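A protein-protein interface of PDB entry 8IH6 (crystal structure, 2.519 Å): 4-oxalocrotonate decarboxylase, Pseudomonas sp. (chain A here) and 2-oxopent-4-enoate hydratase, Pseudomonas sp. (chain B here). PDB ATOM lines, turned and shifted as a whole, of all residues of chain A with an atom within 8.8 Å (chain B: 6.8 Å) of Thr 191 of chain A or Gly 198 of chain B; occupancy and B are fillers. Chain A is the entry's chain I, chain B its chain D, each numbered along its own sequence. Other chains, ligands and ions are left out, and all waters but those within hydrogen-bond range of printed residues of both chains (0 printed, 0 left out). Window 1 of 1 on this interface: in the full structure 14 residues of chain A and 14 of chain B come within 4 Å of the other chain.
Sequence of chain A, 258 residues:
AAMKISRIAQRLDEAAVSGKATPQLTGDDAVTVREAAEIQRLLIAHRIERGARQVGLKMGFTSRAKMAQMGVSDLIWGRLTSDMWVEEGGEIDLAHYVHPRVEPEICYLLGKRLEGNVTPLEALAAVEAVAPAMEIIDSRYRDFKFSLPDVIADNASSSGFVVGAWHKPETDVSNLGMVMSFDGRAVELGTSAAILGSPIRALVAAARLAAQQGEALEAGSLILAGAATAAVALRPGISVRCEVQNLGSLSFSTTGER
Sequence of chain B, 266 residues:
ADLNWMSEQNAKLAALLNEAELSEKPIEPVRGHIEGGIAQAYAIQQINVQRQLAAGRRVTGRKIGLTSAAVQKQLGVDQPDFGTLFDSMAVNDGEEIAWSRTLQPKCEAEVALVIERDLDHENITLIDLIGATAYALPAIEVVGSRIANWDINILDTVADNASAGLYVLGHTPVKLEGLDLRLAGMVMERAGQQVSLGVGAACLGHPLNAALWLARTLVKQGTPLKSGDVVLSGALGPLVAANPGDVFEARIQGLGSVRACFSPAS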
ATOM      1  N   PRO A 104      -6.601  -4.828 -15.586  1.00  0.00           N
ATOM      2  CA  PRO A 104      -5.322  -4.489 -16.196  1.00  0.00           C
ATOM      3  C   PRO A 104      -4.290  -4.227 -15.101  1.00  0.00           C
ATOM      4  O   PRO A 104      -4.624  -3.626 -14.156  1.00  0.00           O
ATOM      5  CB  PRO A 104      -5.667  -3.187 -16.884  1.00  0.00           C
ATOM      6  CG  PRO A 104      -6.588  -2.561 -15.927  1.00  0.00           C
ATOM      7  CD  PRO A 104      -7.493  -3.694 -15.534  1.00  0.00           C
ATOM      8  N   GLU A 105      -3.072  -4.744 -15.250  1.00  0.00           N
ATOM      9  CA  GLU A 105      -2.060  -4.581 -14.180  1.00  0.00           C
ATOM     10  C   GLU A 105      -0.676  -4.301 -14.750  1.00  0.00           C
ATOM     11  O   GLU A 105      -0.522  -4.359 -15.934  1.00  0.00           O
ATOM     12  CB  GLU A 105      -1.861  -5.903 -13.442  1.00  0.00           C
ATOM     13  CG  GLU A 105      -3.117  -6.539 -12.936  1.00  0.00           C
ATOM     14  CD  GLU A 105      -3.029  -6.888 -11.484  1.00  0.00           C
ATOM     15  OE1 GLU A 105      -1.969  -6.753 -10.933  1.00  0.00           O
ATOM     16  OE2 GLU A 105      -4.029  -7.295 -10.941  1.00  0.00           O
ATOM     17  N   ILE A 106       0.278  -4.039 -13.866  1.00  0.00           N
ATOM     18  CA  ILE A 106       1.704  -3.862 -14.240  1.00  0.00           C
ATOM     19  C   ILE A 106       2.411  -5.045 -13.601  1.00  0.00           C
ATOM     20  O   ILE A 106       2.121  -5.315 -12.474  1.00  0.00           O
ATOM     21  CB  ILE A 106       2.269  -2.517 -13.762  1.00  0.00           C
ATOM     22  CG1 ILE A 106       1.698  -1.354 -14.562  1.00  0.00           C
ATOM     23  CG2 ILE A 106       3.774  -2.514 -13.816  1.00  0.00           C
ATOM     24  CD1 ILE A 106       1.596  -1.609 -16.022  1.00  0.00           C
ATOM     25  N   VAL A 173       6.916   3.622 -14.974  1.00  0.00           N
ATOM     26  CA  VAL A 173       5.566   3.006 -15.011  1.00  0.00           C
ATOM     27  C   VAL A 173       4.647   3.695 -14.011  1.00  0.00           C
ATOM     28  O   VAL A 173       3.542   3.267 -13.847  1.00  0.00           O
ATOM     29  CB  VAL A 173       5.689   1.500 -14.734  1.00  0.00           C
ATOM     30  CG1 VAL A 173       6.386   0.786 -15.871  1.00  0.00           C
ATOM     31  CG2 VAL A 173       6.400   1.236 -13.427  1.00  0.00           C
ATOM     32  N   SER A 174       5.106   4.798 -13.462  1.00  0.00           N
ATOM     33  CA  SER A 174       4.406   5.578 -12.423  1.00  0.00           C
ATOM     34  C   SER A 174       3.078   6.149 -12.901  1.00  0.00           C
ATOM     35  O   SER A 174       2.189   6.231 -12.106  1.00  0.00           O
ATOM     36  CB  SER A 174       5.283   6.656 -11.957  1.00  0.00           C
ATOM     37  OG  SER A 174       5.168   7.756 -12.823  1.00  0.00           O
ATOM     38  N   ASN A 175       2.953   6.531 -14.155  1.00  0.00           N
ATOM     39  CA  ASN A 175       1.670   7.122 -14.587  1.00  0.00           C
ATOM     40  C   ASN A 175       1.429   6.820 -16.055  1.00  0.00           C
ATOM     41  O   ASN A 175       1.246   7.730 -16.788  1.00  0.00           O
ATOM     42  CB  ASN A 175       1.621   8.611 -14.268  1.00  0.00           C
ATOM     43  CG  ASN A 175       0.401   9.325 -14.790  1.00  0.00           C
ATOM     44  OD1 ASN A 175      -0.677   8.782 -14.802  1.00  0.00           O
ATOM     45  ND2 ASN A 175       0.573  10.543 -15.239  1.00  0.00           N
ATOM     46  N   LEU A 176       1.365   5.551 -16.428  1.00  0.00           N
ATOM     47  CA  LEU A 176       1.111   5.173 -17.836  1.00  0.00           C
ATOM     48  C   LEU A 176      -0.378   4.971 -18.082  1.00  0.00           C
ATOM     49  O   LEU A 176      -1.051   4.356 -17.282  1.00  0.00           O
ATOM     50  CB  LEU A 176       1.874   3.897 -18.169  1.00  0.00           C
ATOM     51  CG  LEU A 176       3.359   3.917 -17.861  1.00  0.00           C
ATOM     52  CD1 LEU A 176       4.010   2.642 -18.308  1.00  0.00           C
ATOM     53  CD2 LEU A 176       4.017   5.092 -18.534  1.00  0.00           C
ATOM     54  N   GLY A 177      -0.854   5.427 -19.223  1.00  0.00           N
ATOM     55  CA  GLY A 177      -2.268   5.252 -19.551  1.00  0.00           C
ATOM     56  C   GLY A 177      -2.589   3.810 -19.834  1.00  0.00           C
ATOM     57  O   GLY A 177      -1.746   3.093 -20.284  1.00  0.00           O
ATOM     58  N   MET A 178      -3.821   3.417 -19.594  1.00  0.00           N
ATOM     59  CA  MET A 178      -4.173   2.008 -19.808  1.00  0.00           C
ATOM     60  C   MET A 178      -5.530   1.958 -20.471  1.00  0.00           C
ATOM     61  O   MET A 178      -6.362   2.716 -20.103  1.00  0.00           O
ATOM     62  CB  MET A 178      -4.253   1.294 -18.463  1.00  0.00           C
ATOM     63  CG  MET A 178      -3.222   0.227 -18.297  1.00  0.00           C
ATOM     64  SD  MET A 178      -2.587   0.081 -16.645  1.00  0.00           S
ATOM     65  CE  MET A 178      -1.804  -1.511 -16.762  1.00  0.00           C
ATOM     66  N   VAL A 179      -5.668   1.147 -21.494  1.00  0.00           N
ATOM     67  CA  VAL A 179      -6.992   0.968 -22.134  1.00  0.00           C
ATOM     68  C   VAL A 179      -7.272  -0.533 -22.166  1.00  0.00           C
ATOM     69  O   VAL A 179      -6.533  -1.243 -22.792  1.00  0.00           O
ATOM     70  CB  VAL A 179      -7.061   1.606 -23.530  1.00  0.00           C
ATOM     71  CG1 VAL A 179      -8.335   1.216 -24.235  1.00  0.00           C
ATOM     72  CG2 VAL A 179      -6.971   3.108 -23.443  1.00  0.00           C
ATOM     73  N   GLU A 188     -12.654  -0.244 -19.811  1.00  0.00           N
ATOM     74  CA  GLU A 188     -12.095   0.511 -18.669  1.00  0.00           C
ATOM     75  C   GLU A 188     -10.962   1.420 -19.134  1.00  0.00           C
ATOM     76  O   GLU A 188     -10.236   1.035 -20.020  1.00  0.00           O
ATOM     77  CB  GLU A 188     -11.652  -0.431 -17.563  1.00  0.00           C
ATOM     78  CG  GLU A 188     -12.797  -0.934 -16.729  1.00  0.00           C
ATOM     79  CD  GLU A 188     -13.539   0.103 -15.928  1.00  0.00           C
ATOM     80  OE1 GLU A 188     -12.895   0.998 -15.407  1.00  0.00           O
ATOM     81  OE2 GLU A 188     -14.750  -0.024 -15.810  1.00  0.00           O
ATOM     82  N   LEU A 189     -10.863   2.594 -18.526  1.00  0.00           N
ATOM     83  CA  LEU A 189      -9.847   3.609 -18.887  1.00  0.00           C
ATOM     84  C   LEU A 189      -9.128   4.039 -17.621  1.00  0.00           C
ATOM     85  O   LEU A 189      -9.792   4.280 -16.654  1.00  0.00           O
ATOM     86  CB  LEU A 189     -10.568   4.795 -19.518  1.00  0.00           C
ATOM     87  CG  LEU A 189     -11.014   4.574 -20.953  1.00  0.00           C
ATOM     88  CD1 LEU A 189     -11.624   5.821 -21.531  1.00  0.00           C
ATOM     89  CD2 LEU A 189      -9.856   4.120 -21.799  1.00  0.00           C
ATOM     90  N   GLY A 190      -7.810   4.126 -17.648  1.00  0.00           N
ATOM     91  CA  GLY A 190      -7.119   4.563 -16.432  1.00  0.00           C
ATOM     92  C   GLY A 190      -5.634   4.683 -16.621  1.00  0.00           C
ATOM     93  O   GLY A 190      -5.214   4.696 -17.733  1.00  0.00           O
ATOM     94  N   THR A 191      -4.913   4.710 -15.529  1.00  0.00           N
ATOM     95  CA  THR A 191      -3.464   4.893 -15.595  1.00  0.00           C
ATOM     96  C   THR A 191      -2.817   3.921 -14.632  1.00  0.00           C
ATOM     97  O   THR A 191      -3.433   3.550 -13.687  1.00  0.00           O
ATOM     98  CB  THR A 191      -3.123   6.322 -15.162  1.00  0.00           C
ATOM     99  OG1 THR A 191      -1.757   6.377 -14.780  1.00  0.00           O
ATOM    100  CG2 THR A 191      -3.954   6.808 -14.004  1.00  0.00           C
ATOM    101  N   SER A 192      -1.574   3.536 -14.854  1.00  0.00           N
ATOM    102  CA  SER A 192      -0.954   2.624 -13.869  1.00  0.00           C
ATOM    103  C   SER A 192      -0.687   3.389 -12.580  1.00  0.00           C
ATOM    104  O   SER A 192      -0.243   2.807 -11.619  1.00  0.00           O
ATOM    105  CB  SER A 192       0.276   2.047 -14.401  1.00  0.00           C
ATOM    106  OG  SER A 192       1.181   3.064 -14.670  1.00  0.00           O
ATOM    107  N   ALA A 193      -0.993   4.674 -12.583  1.00  0.00           N
ATOM    108  CA  ALA A 193      -0.780   5.470 -11.366  1.00  0.00           C
ATOM    109  C   ALA A 193      -1.825   5.086 -10.326  1.00  0.00           C
ATOM    110  O   ALA A 193      -1.650   5.418  -9.172  1.00  0.00           O
ATOM    111  CB  ALA A 193      -0.835   6.923 -11.693  1.00  0.00           C
ATOM    112  N   ALA A 194      -2.850   4.362 -10.758  1.00  0.00           N
ATOM    113  CA  ALA A 194      -3.923   3.901  -9.857  1.00  0.00           C
ATOM    114  C   ALA A 194      -3.363   2.887  -8.872  1.00  0.00           C
ATOM    115  O   ALA A 194      -3.981   2.658  -7.868  1.00  0.00           O
ATOM    116  CB  ALA A 194      -5.060   3.319 -10.641  1.00  0.00           C
ATOM    117  N   ILE A 195      -2.257   2.250  -9.202  1.00  0.00           N
ATOM    118  CA  ILE A 195      -1.679   1.225  -8.299  1.00  0.00           C
ATOM    119  C   ILE A 195      -0.847   1.923  -7.240  1.00  0.00           C
ATOM    120  O   ILE A 195       0.283   2.225  -7.526  1.00  0.00           O
ATOM    121  CB  ILE A 195      -0.829   0.229  -9.092  1.00  0.00           C
ATOM    122  CG1 ILE A 195      -1.680  -0.580 -10.054  1.00  0.00           C
ATOM    123  CG2 ILE A 195      -0.039  -0.658  -8.164  1.00  0.00           C
ATOM    124  CD1 ILE A 195      -0.869  -1.272 -11.084  1.00  0.00           C
ATOM    125  N   LEU A 196      -1.459   2.243  -6.102  1.00  0.00           N
ATOM    126  CA  LEU A 196      -0.832   2.892  -4.922  1.00  0.00           C
ATOM    127  C   LEU A 196      -0.193   4.238  -5.244  1.00  0.00           C
ATOM    128  O   LEU A 196       0.609   4.658  -4.463  1.00  0.00           O
ATOM    129  CB  LEU A 196       0.215   1.964  -4.325  1.00  0.00           C
ATOM    130  CG  LEU A 196      -0.316   0.859  -3.436  1.00  0.00           C
ATOM    131  CD1 LEU A 196       0.820   0.195  -2.705  1.00  0.00           C
ATOM    132  CD2 LEU A 196      -1.318   1.416  -2.462  1.00  0.00           C
ATOM    133  N   GLY A 197      -0.541   4.889  -6.344  1.00  0.00           N
ATOM    134  CA  GLY A 197       0.102   6.174  -6.662  1.00  0.00           C
ATOM    135  C   GLY A 197       1.417   5.987  -7.390  1.00  0.00           C
ATOM    136  O   GLY A 197       1.870   6.919  -7.983  1.00  0.00           O
ATOM    137  N   SER A 198       2.009   4.812  -7.321  1.00  0.00           N
ATOM    138  CA  SER A 198       3.270   4.490  -8.030  1.00  0.00           C
ATOM    139  C   SER A 198       3.407   2.977  -7.986  1.00  0.00           C
ATOM    140  O   SER A 198       3.631   2.504  -6.939  1.00  0.00           O
ATOM    141  CB  SER A 198       4.449   5.126  -7.362  1.00  0.00           C
ATOM    142  OG  SER A 198       5.599   4.993  -8.163  1.00  0.00           O
ATOM    143  N   PRO A 199       3.338   2.202  -9.077  1.00  0.00           N
ATOM    144  CA  PRO A 199       3.435   0.757  -8.991  1.00  0.00           C
ATOM    145  C   PRO A 199       4.557   0.134  -8.160  1.00  0.00           C
ATOM    146  O   PRO A 199       4.346  -0.861  -7.632  1.00  0.00           O
ATOM    147  CB  PRO A 199       3.509   0.357 -10.453  1.00  0.00           C
ATOM    148  CG  PRO A 199       2.637   1.358 -11.106  1.00  0.00           C
ATOM    149  CD  PRO A 199       3.034   2.638 -10.416  1.00  0.00           C
ATOM    150  N   GLY A 226      -0.973  -4.877  -9.166  1.00  0.00           N
ATOM    151  CA  GLY A 226      -2.282  -4.435  -8.672  1.00  0.00           C
ATOM    152  C   GLY A 226      -3.158  -3.948  -9.787  1.00  0.00           C
ATOM    153  O   GLY A 226      -2.655  -3.726 -10.844  1.00  0.00           O
ATOM    154  N   ALA A 227      -4.438  -3.763  -9.540  1.00  0.00           N
ATOM    155  CA  ALA A 227      -5.345  -3.379 -10.642  1.00  0.00           C
ATOM    156  C   ALA A 227      -5.372  -1.881 -10.897  1.00  0.00           C
ATOM    157  O   ALA A 227      -5.615  -1.168 -10.013  1.00  0.00           O
ATOM    158  CB  ALA A 227      -6.726  -3.896 -10.396  1.00  0.00           C
ATOM    159  N   ALA A 228      -5.149  -1.466 -12.125  1.00  0.00           N
ATOM    160  CA  ALA A 228      -5.173  -0.033 -12.446  1.00  0.00           C
ATOM    161  C   ALA A 228      -6.622   0.397 -12.619  1.00  0.00           C
ATOM    162  O   ALA A 228      -6.924   1.533 -12.387  1.00  0.00           O
ATOM    163  CB  ALA A 228      -4.355   0.224 -13.675  1.00  0.00           C
ATOM    164  N   THR A 229      -7.488  -0.514 -13.029  1.00  0.00           N
ATOM    165  CA  THR A 229      -8.917  -0.148 -13.134  1.00  0.00           C
ATOM    166  C   THR A 229      -9.764  -1.167 -12.392  1.00  0.00           C
ATOM    167  O   THR A 229      -9.229  -2.121 -11.866  1.00  0.00           O
ATOM    168  CB  THR A 229      -9.445  -0.095 -14.568  1.00  0.00           C
ATOM    169  OG1 THR A 229      -9.444  -1.387 -15.147  1.00  0.00           O
ATOM    170  CG2 THR A 229      -8.660   0.833 -15.450  1.00  0.00           C
ATOM    171  N   GLU A 243      -3.866  -2.235 -23.447  1.00  0.00           N
ATOM    172  CA  GLU A 243      -2.878  -1.381 -24.137  1.00  0.00           C
ATOM    173  C   GLU A 243      -2.309  -0.410 -23.122  1.00  0.00           C
ATOM    174  O   GLU A 243      -3.078   0.191 -22.436  1.00  0.00           O
ATOM    175  CB  GLU A 243      -3.581  -0.670 -25.282  1.00  0.00           C
ATOM    176  CG  GLU A 243      -2.659   0.167 -26.123  1.00  0.00           C
ATOM    177  CD  GLU A 243      -3.282   0.470 -27.455  1.00  0.00           C
ATOM    178  OE1 GLU A 243      -2.549   0.677 -28.392  1.00  0.00           O
ATOM    179  OE2 GLU A 243      -4.491   0.461 -27.521  1.00  0.00           O
ATOM    180  N   VAL A 244      -0.991  -0.307 -22.990  1.00  0.00           N
ATOM    181  CA  VAL A 244      -0.413   0.614 -21.972  1.00  0.00           C
ATOM    182  C   VAL A 244       0.579   1.568 -22.630  1.00  0.00           C
ATOM    183  O   VAL A 244       1.323   1.137 -23.492  1.00  0.00           O
ATOM    184  CB  VAL A 244       0.218  -0.149 -20.799  1.00  0.00           C
ATOM    185  CG1 VAL A 244       0.680   0.764 -19.694  1.00  0.00           C
ATOM    186  CG2 VAL A 244      -0.731  -1.163 -20.222  1.00  0.00           C
ATOM    187  N   GLN A 245       0.569   2.825 -22.195  1.00  0.00           N
ATOM    188  CA  GLN A 245       1.471   3.868 -22.711  1.00  0.00           C
ATOM    189  C   GLN A 245       2.901   3.411 -22.475  1.00  0.00           C
ATOM    190  O   GLN A 245       3.186   3.027 -21.360  1.00  0.00           O
ATOM    191  CB  GLN A 245       1.216   5.189 -22.005  1.00  0.00           C
ATOM    192  CG  GLN A 245       2.118   6.295 -22.500  1.00  0.00           C
ATOM    193  CD  GLN A 245       1.905   7.591 -21.780  1.00  0.00           C
ATOM    194  OE1 GLN A 245       1.603   7.615 -20.608  1.00  0.00           O
ATOM    195  NE2 GLN A 245       2.063   8.681 -22.486  1.00  0.00           N
ATOM    196  N   LEU B 183      -2.927   7.737 -25.191  1.00  0.00           N
ATOM    197  CA  LEU B 183      -2.640   6.867 -24.039  1.00  0.00           C
ATOM    198  C   LEU B 183      -1.927   7.630 -22.942  1.00  0.00           C
ATOM    199  O   LEU B 183      -1.431   6.982 -22.067  1.00  0.00           O
ATOM    200  CB  LEU B 183      -1.786   5.695 -24.496  1.00  0.00           C
ATOM    201  CG  LEU B 183      -2.355   4.912 -25.666  1.00  0.00           C
ATOM    202  CD1 LEU B 183      -1.358   3.885 -26.129  1.00  0.00           C
ATOM    203  CD2 LEU B 183      -3.653   4.257 -25.289  1.00  0.00           C
ATOM    204  N   ALA B 184      -1.938   8.954 -22.980  1.00  0.00           N
ATOM    205  CA  ALA B 184      -1.259   9.730 -21.925  1.00  0.00           C
ATOM    206  C   ALA B 184      -1.963   9.510 -20.592  1.00  0.00           C
ATOM    207  O   ALA B 184      -3.147   9.793 -20.482  1.00  0.00           O
ATOM    208  CB  ALA B 184      -1.213  11.187 -22.285  1.00  0.00           C
ATOM    209  N   GLY B 185      -1.219   9.039 -19.610  1.00  0.00           N
ATOM    210  CA  GLY B 185      -1.787   8.754 -18.294  1.00  0.00           C
ATOM    211  C   GLY B 185      -1.991  10.001 -17.485  1.00  0.00           C
ATOM    212  O   GLY B 185      -1.185  10.896 -17.590  1.00  0.00           O
ATOM    213  N   MET B 186      -3.050  10.033 -16.686  1.00  0.00           N
ATOM    214  CA  MET B 186      -3.309  11.207 -15.836  1.00  0.00           C
ATOM    215  C   MET B 186      -3.541  10.803 -14.387  1.00  0.00           C
ATOM    216  O   MET B 186      -4.253   9.864 -14.143  1.00  0.00           O
ATOM    217  CB  MET B 186      -4.502  12.017 -16.328  1.00  0.00           C
ATOM    218  CG  MET B 186      -4.709  13.281 -15.537  1.00  0.00           C
ATOM    219  SD  MET B 186      -5.540  13.095 -13.973  1.00  0.00           S
ATOM    220  CE  MET B 186      -7.180  12.697 -14.528  1.00  0.00           C
ATOM    221  N   VAL B 187      -2.897  11.526 -13.492  1.00  0.00           N
ATOM    222  CA  VAL B 187      -3.099  11.370 -12.036  1.00  0.00           C
ATOM    223  C   VAL B 187      -3.172  12.777 -11.436  1.00  0.00           C
ATOM    224  O   VAL B 187      -2.418  13.639 -11.838  1.00  0.00           O
ATOM    225  CB  VAL B 187      -2.044  10.474 -11.367  1.00  0.00           C
ATOM    226  CG1 VAL B 187      -0.637  10.991 -11.562  1.00  0.00           C
ATOM    227  CG2 VAL B 187      -2.348  10.292  -9.899  1.00  0.00           C
ATOM    228  N   MET B 188      -4.164  13.018 -10.600  1.00  0.00           N
ATOM    229  CA  MET B 188      -4.250  14.305  -9.898  1.00  0.00           C
ATOM    230  C   MET B 188      -4.191  13.957  -8.430  1.00  0.00           C
ATOM    231  O   MET B 188      -4.889  13.088  -8.042  1.00  0.00           O
ATOM    232  CB  MET B 188      -5.543  15.052 -10.194  1.00  0.00           C
ATOM    233  CG  MET B 188      -5.589  16.398  -9.524  1.00  0.00           C
ATOM    234  SD  MET B 188      -6.571  17.583 -10.384  1.00  0.00           S
ATOM    235  CE  MET B 188      -8.146  16.752 -10.422  1.00  0.00           C
ATOM    236  N   SER B 196      -7.875  11.874  -8.622  1.00  0.00           N
ATOM    237  CA  SER B 196      -8.405  11.713 -10.002  1.00  0.00           C
ATOM    238  C   SER B 196      -7.470  10.854 -10.841  1.00  0.00           C
ATOM    239  O   SER B 196      -6.299  11.037 -10.765  1.00  0.00           O
ATOM    240  CB  SER B 196      -8.689  13.000 -10.682  1.00  0.00           C
ATOM    241  OG  SER B 196      -9.811  12.884 -11.525  1.00  0.00           O
ATOM    242  N   LEU B 197      -8.028   9.927 -11.597  1.00  0.00           N
ATOM    243  CA  LEU B 197      -7.220   9.024 -12.429  1.00  0.00           C
ATOM    244  C   LEU B 197      -7.804   9.029 -13.826  1.00  0.00           C
ATOM    245  O   LEU B 197      -9.003   9.046 -13.953  1.00  0.00           O
ATOM    246  CB  LEU B 197      -7.237   7.637 -11.808  1.00  0.00           C
ATOM    247  CG  LEU B 197      -6.406   7.534 -10.547  1.00  0.00           C
ATOM    248  CD1 LEU B 197      -6.879   6.401  -9.681  1.00  0.00           C
ATOM    249  CD2 LEU B 197      -4.951   7.373 -10.883  1.00  0.00           C
ATOM    250  N   GLY B 198      -6.944   9.047 -14.831  1.00  0.00           N
ATOM    251  CA  GLY B 198      -7.463   9.094 -16.197  1.00  0.00           C
ATOM    252  C   GLY B 198      -6.421   8.809 -17.239  1.00  0.00           C
ATOM    253  O   GLY B 198      -5.348   8.414 -16.907  1.00  0.00           O
ATOM    254  N   VAL B 199      -6.798   9.042 -18.476  1.00  0.00           N
ATOM    255  CA  VAL B 199      -5.940   8.821 -19.661  1.00  0.00           C
ATOM    256  C   VAL B 199      -6.441   9.772 -20.746  1.00  0.00           C
ATOM    257  O   VAL B 199      -7.584  10.145 -20.717  1.00  0.00           O
ATOM    258  CB  VAL B 199      -5.996   7.340 -20.073  1.00  0.00           C
ATOM    259  CG1 VAL B 199      -7.372   6.908 -20.507  1.00  0.00           C
ATOM    260  CG2 VAL B 199      -4.965   6.960 -21.100  1.00  0.00           C
ATOM    261  N   GLY B 200      -5.585  10.107 -21.700  1.00  0.00           N
ATOM    262  CA  GLY B 200      -5.975  11.050 -22.753  1.00  0.00           C
ATOM    263  C   GLY B 200      -7.200  10.613 -23.510  1.00  0.00           C
ATOM    264  O   GLY B 200      -7.935  11.468 -23.942  1.00  0.00           O
ATOM    265  N   ALA B 201      -7.403   9.307 -23.631  1.00  0.00           N
ATOM    266  CA  ALA B 201      -8.500   8.697 -24.409  1.00  0.00           C
ATOM    267  C   ALA B 201      -9.865   8.985 -23.794  1.00  0.00           C
ATOM    268  O   ALA B 201     -10.845   8.928 -24.499  1.00  0.00           O
ATOM    269  CB  ALA B 201      -8.239   7.232 -24.521  1.00  0.00           C
ATOM    270  N   ALA B 202      -9.887   9.329 -22.516  1.00  0.00           N
ATOM    271  CA  ALA B 202     -11.143   9.605 -21.792  1.00  0.00           C
ATOM    272  C   ALA B 202     -11.762  10.901 -22.297  1.00  0.00           C
ATOM    273  O   ALA B 202     -12.952  11.076 -22.161  1.00  0.00           O
ATOM    274  CB  ALA B 202     -10.866   9.683 -20.324  1.00  0.00           C
ATOM    275  N   LEU B 236      -9.926  14.542 -18.223  1.00  0.00           N
ATOM    276  CA  LEU B 236      -9.154  13.308 -18.406  1.00  0.00           C
ATOM    277  C   LEU B 236      -9.579  12.340 -17.297  1.00  0.00           C
ATOM    278  O   LEU B 236      -9.399  11.160 -17.451  1.00  0.00           O
ATOM    279  CB  LEU B 236      -7.677  13.686 -18.298  1.00  0.00           C
ATOM    280  CG  LEU B 236      -7.113  14.445 -19.490  1.00  0.00           C
ATOM    281  CD1 LEU B 236      -5.721  14.961 -19.206  1.00  0.00           C
ATOM    282  CD2 LEU B 236      -7.104  13.572 -20.711  1.00  0.00           C
ATOM    283  N   GLY B 237     -10.151  12.870 -16.228  1.00  0.00           N
ATOM    284  CA  GLY B 237     -10.623  12.091 -15.084  1.00  0.00           C
ATOM    285  C   GLY B 237     -11.743  12.808 -14.369  1.00  0.00           C
ATOM    286  O   GLY B 237     -12.110  13.874 -14.783  1.00  0.00           O
ATOM    287  N   PRO B 238     -12.254  12.280 -13.254  1.00  0.00           N
ATOM    288  CA  PRO B 238     -13.345  12.890 -12.556  1.00  0.00           C
ATOM    289  C   PRO B 238     -12.913  14.119 -11.758  1.00  0.00           C
ATOM    290  O   PRO B 238     -11.836  14.163 -11.314  1.00  0.00           O
ATOM    291  CB  PRO B 238     -13.802  11.787 -11.606  1.00  0.00           C
ATOM    292  CG  PRO B 238     -13.071  10.579 -12.047  1.00  0.00           C
ATOM    293  CD  PRO B 238     -11.777  11.110 -12.591  1.00  0.00           C
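O of Leu 183 of chain B lies close to N of Gly 177 of chain A, at 3.3 Å.
The side-chain amide oxygen of Gln 245 of chain A lies close to the backbone carbonyl oxygen of Leu 183 of chain B, at 3.4 Å.
O of Gly 185 of chain B sits at hydrogen-bond distance from ND2 of Asn 175 of chain A (3.0 Å).
N of Gly 185 of chain B lies within hydrogen-bond range of OE1 of Gln 245 of chain A.
The backbone NH of Met 186 of chain B is in hydrogen-bond range of the side-chain amide oxygen of Asn 175 of chain A (3.3 Å).
The backbone NH (N) of Met 188 of chain B is in hydrogen-bond range of the side-chain sulfur (SD) of Met 186 of chain B.
The backbone NH (N) of Met 186 of chain B sits at hydrogen-bond distance from the backbone carbonyl oxygen (O) of Gly 198 of chain B (2.8 Å).
The side-chain hydroxyl (OG1) of Thr 191 of chain A lies close to the backbone carbonyl oxygen (O) of Leu 176 of chain A.
N of Ala 193 of chain A lies close to OG1 of Thr 191 of chain A, 2.9 Å away.
Gly 177 of chain A touches Gly 185 of chain B.
CA of Gly 177 of chain A touches CG2 of Val 199 of chain B (3.5 Å).
Val 199 of chain B touches Leu 189 of chain A (CG1 to CD2, 3.95 Å).
Gly 190 of chain A touches Val 199 of chain B.
Thr 191 of chain A touches Leu 197 of chain B.
Ala 193 of chain A touches Val 187 of chain B.
Leu 197 of chain B touches Ala 193 of chain A.
NE2 of Gln 245 of chain A touches CA of Ala 184 of chain B (3.5 Å).
Thr 191 of chain A touches just these residues of chain B: Met 186 (3.1 Å), Leu 197 (3.3 Å) and Gly 198 (3.5 Å).
Of chain A, only Gly 190 and Thr 191 come within 4 Å of Gly 198 of chain B.
Of the printed residues of chain B, Gly 190 of chain A touches Gly 198 (3.8 Å) and Val 199 (3.6 Å).
Of the printed residues of chain B, Gly 177 of chain A touches Leu 183 (3.2 Å), Gly 185 (3.6 Å) and Val 199 (3.5 Å).
Of the printed residues of chain B, Gln 245 of chain A touches Leu 183 (3.2 Å), Ala 184 (3.5 Å) and Gly 185 (3.3 Å).
Printed residues of chain B within 4 Å of Glu 243 of chain A: Leu 183 (3.9 Å).
The nearest residue of chain B that does not touch Thr 191 of chain A is Gly 185 of chain B (4.2 Å).
The nearest printed residue of chain A that does not touch Gly 198 of chain B is Asn 175 of chain A (5.1 Å).
The nearest printed residue of chain A that does not touch Ala 184 of chain B is Gly 177 of chain A (4.4 Å).
Of the 16 printed residues of chain B, 9 touch a printed residue of chain A.
Hydrophobic or aromatic side chains of chain B that line the printed part of chain A: Leu 183, Val 187, Leu 197 and Val 199.
Of the 29 printed residues of chain A, 10 touch a printed residue of chain B.
Printed residues of chain A that touch a printed residue of chain B: Asn 175, Gly 177, Val 179, Leu 189, Gly 190, Thr 191, Ala 193, Ala 194, Glu 243 and Gln 245.
Hydrophobic or aromatic side chains of chain A within 4 Å of the printed part of chain B: Val 179, Leu 189, Ala 193 and Ala 194.
Among the printed residues, 21 pairs touch across the chains.
Among the printed residues, no Asp or Glu carboxylate lies within 4 Å of a Lys or Arg side-chain nitrogen of the other chain.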
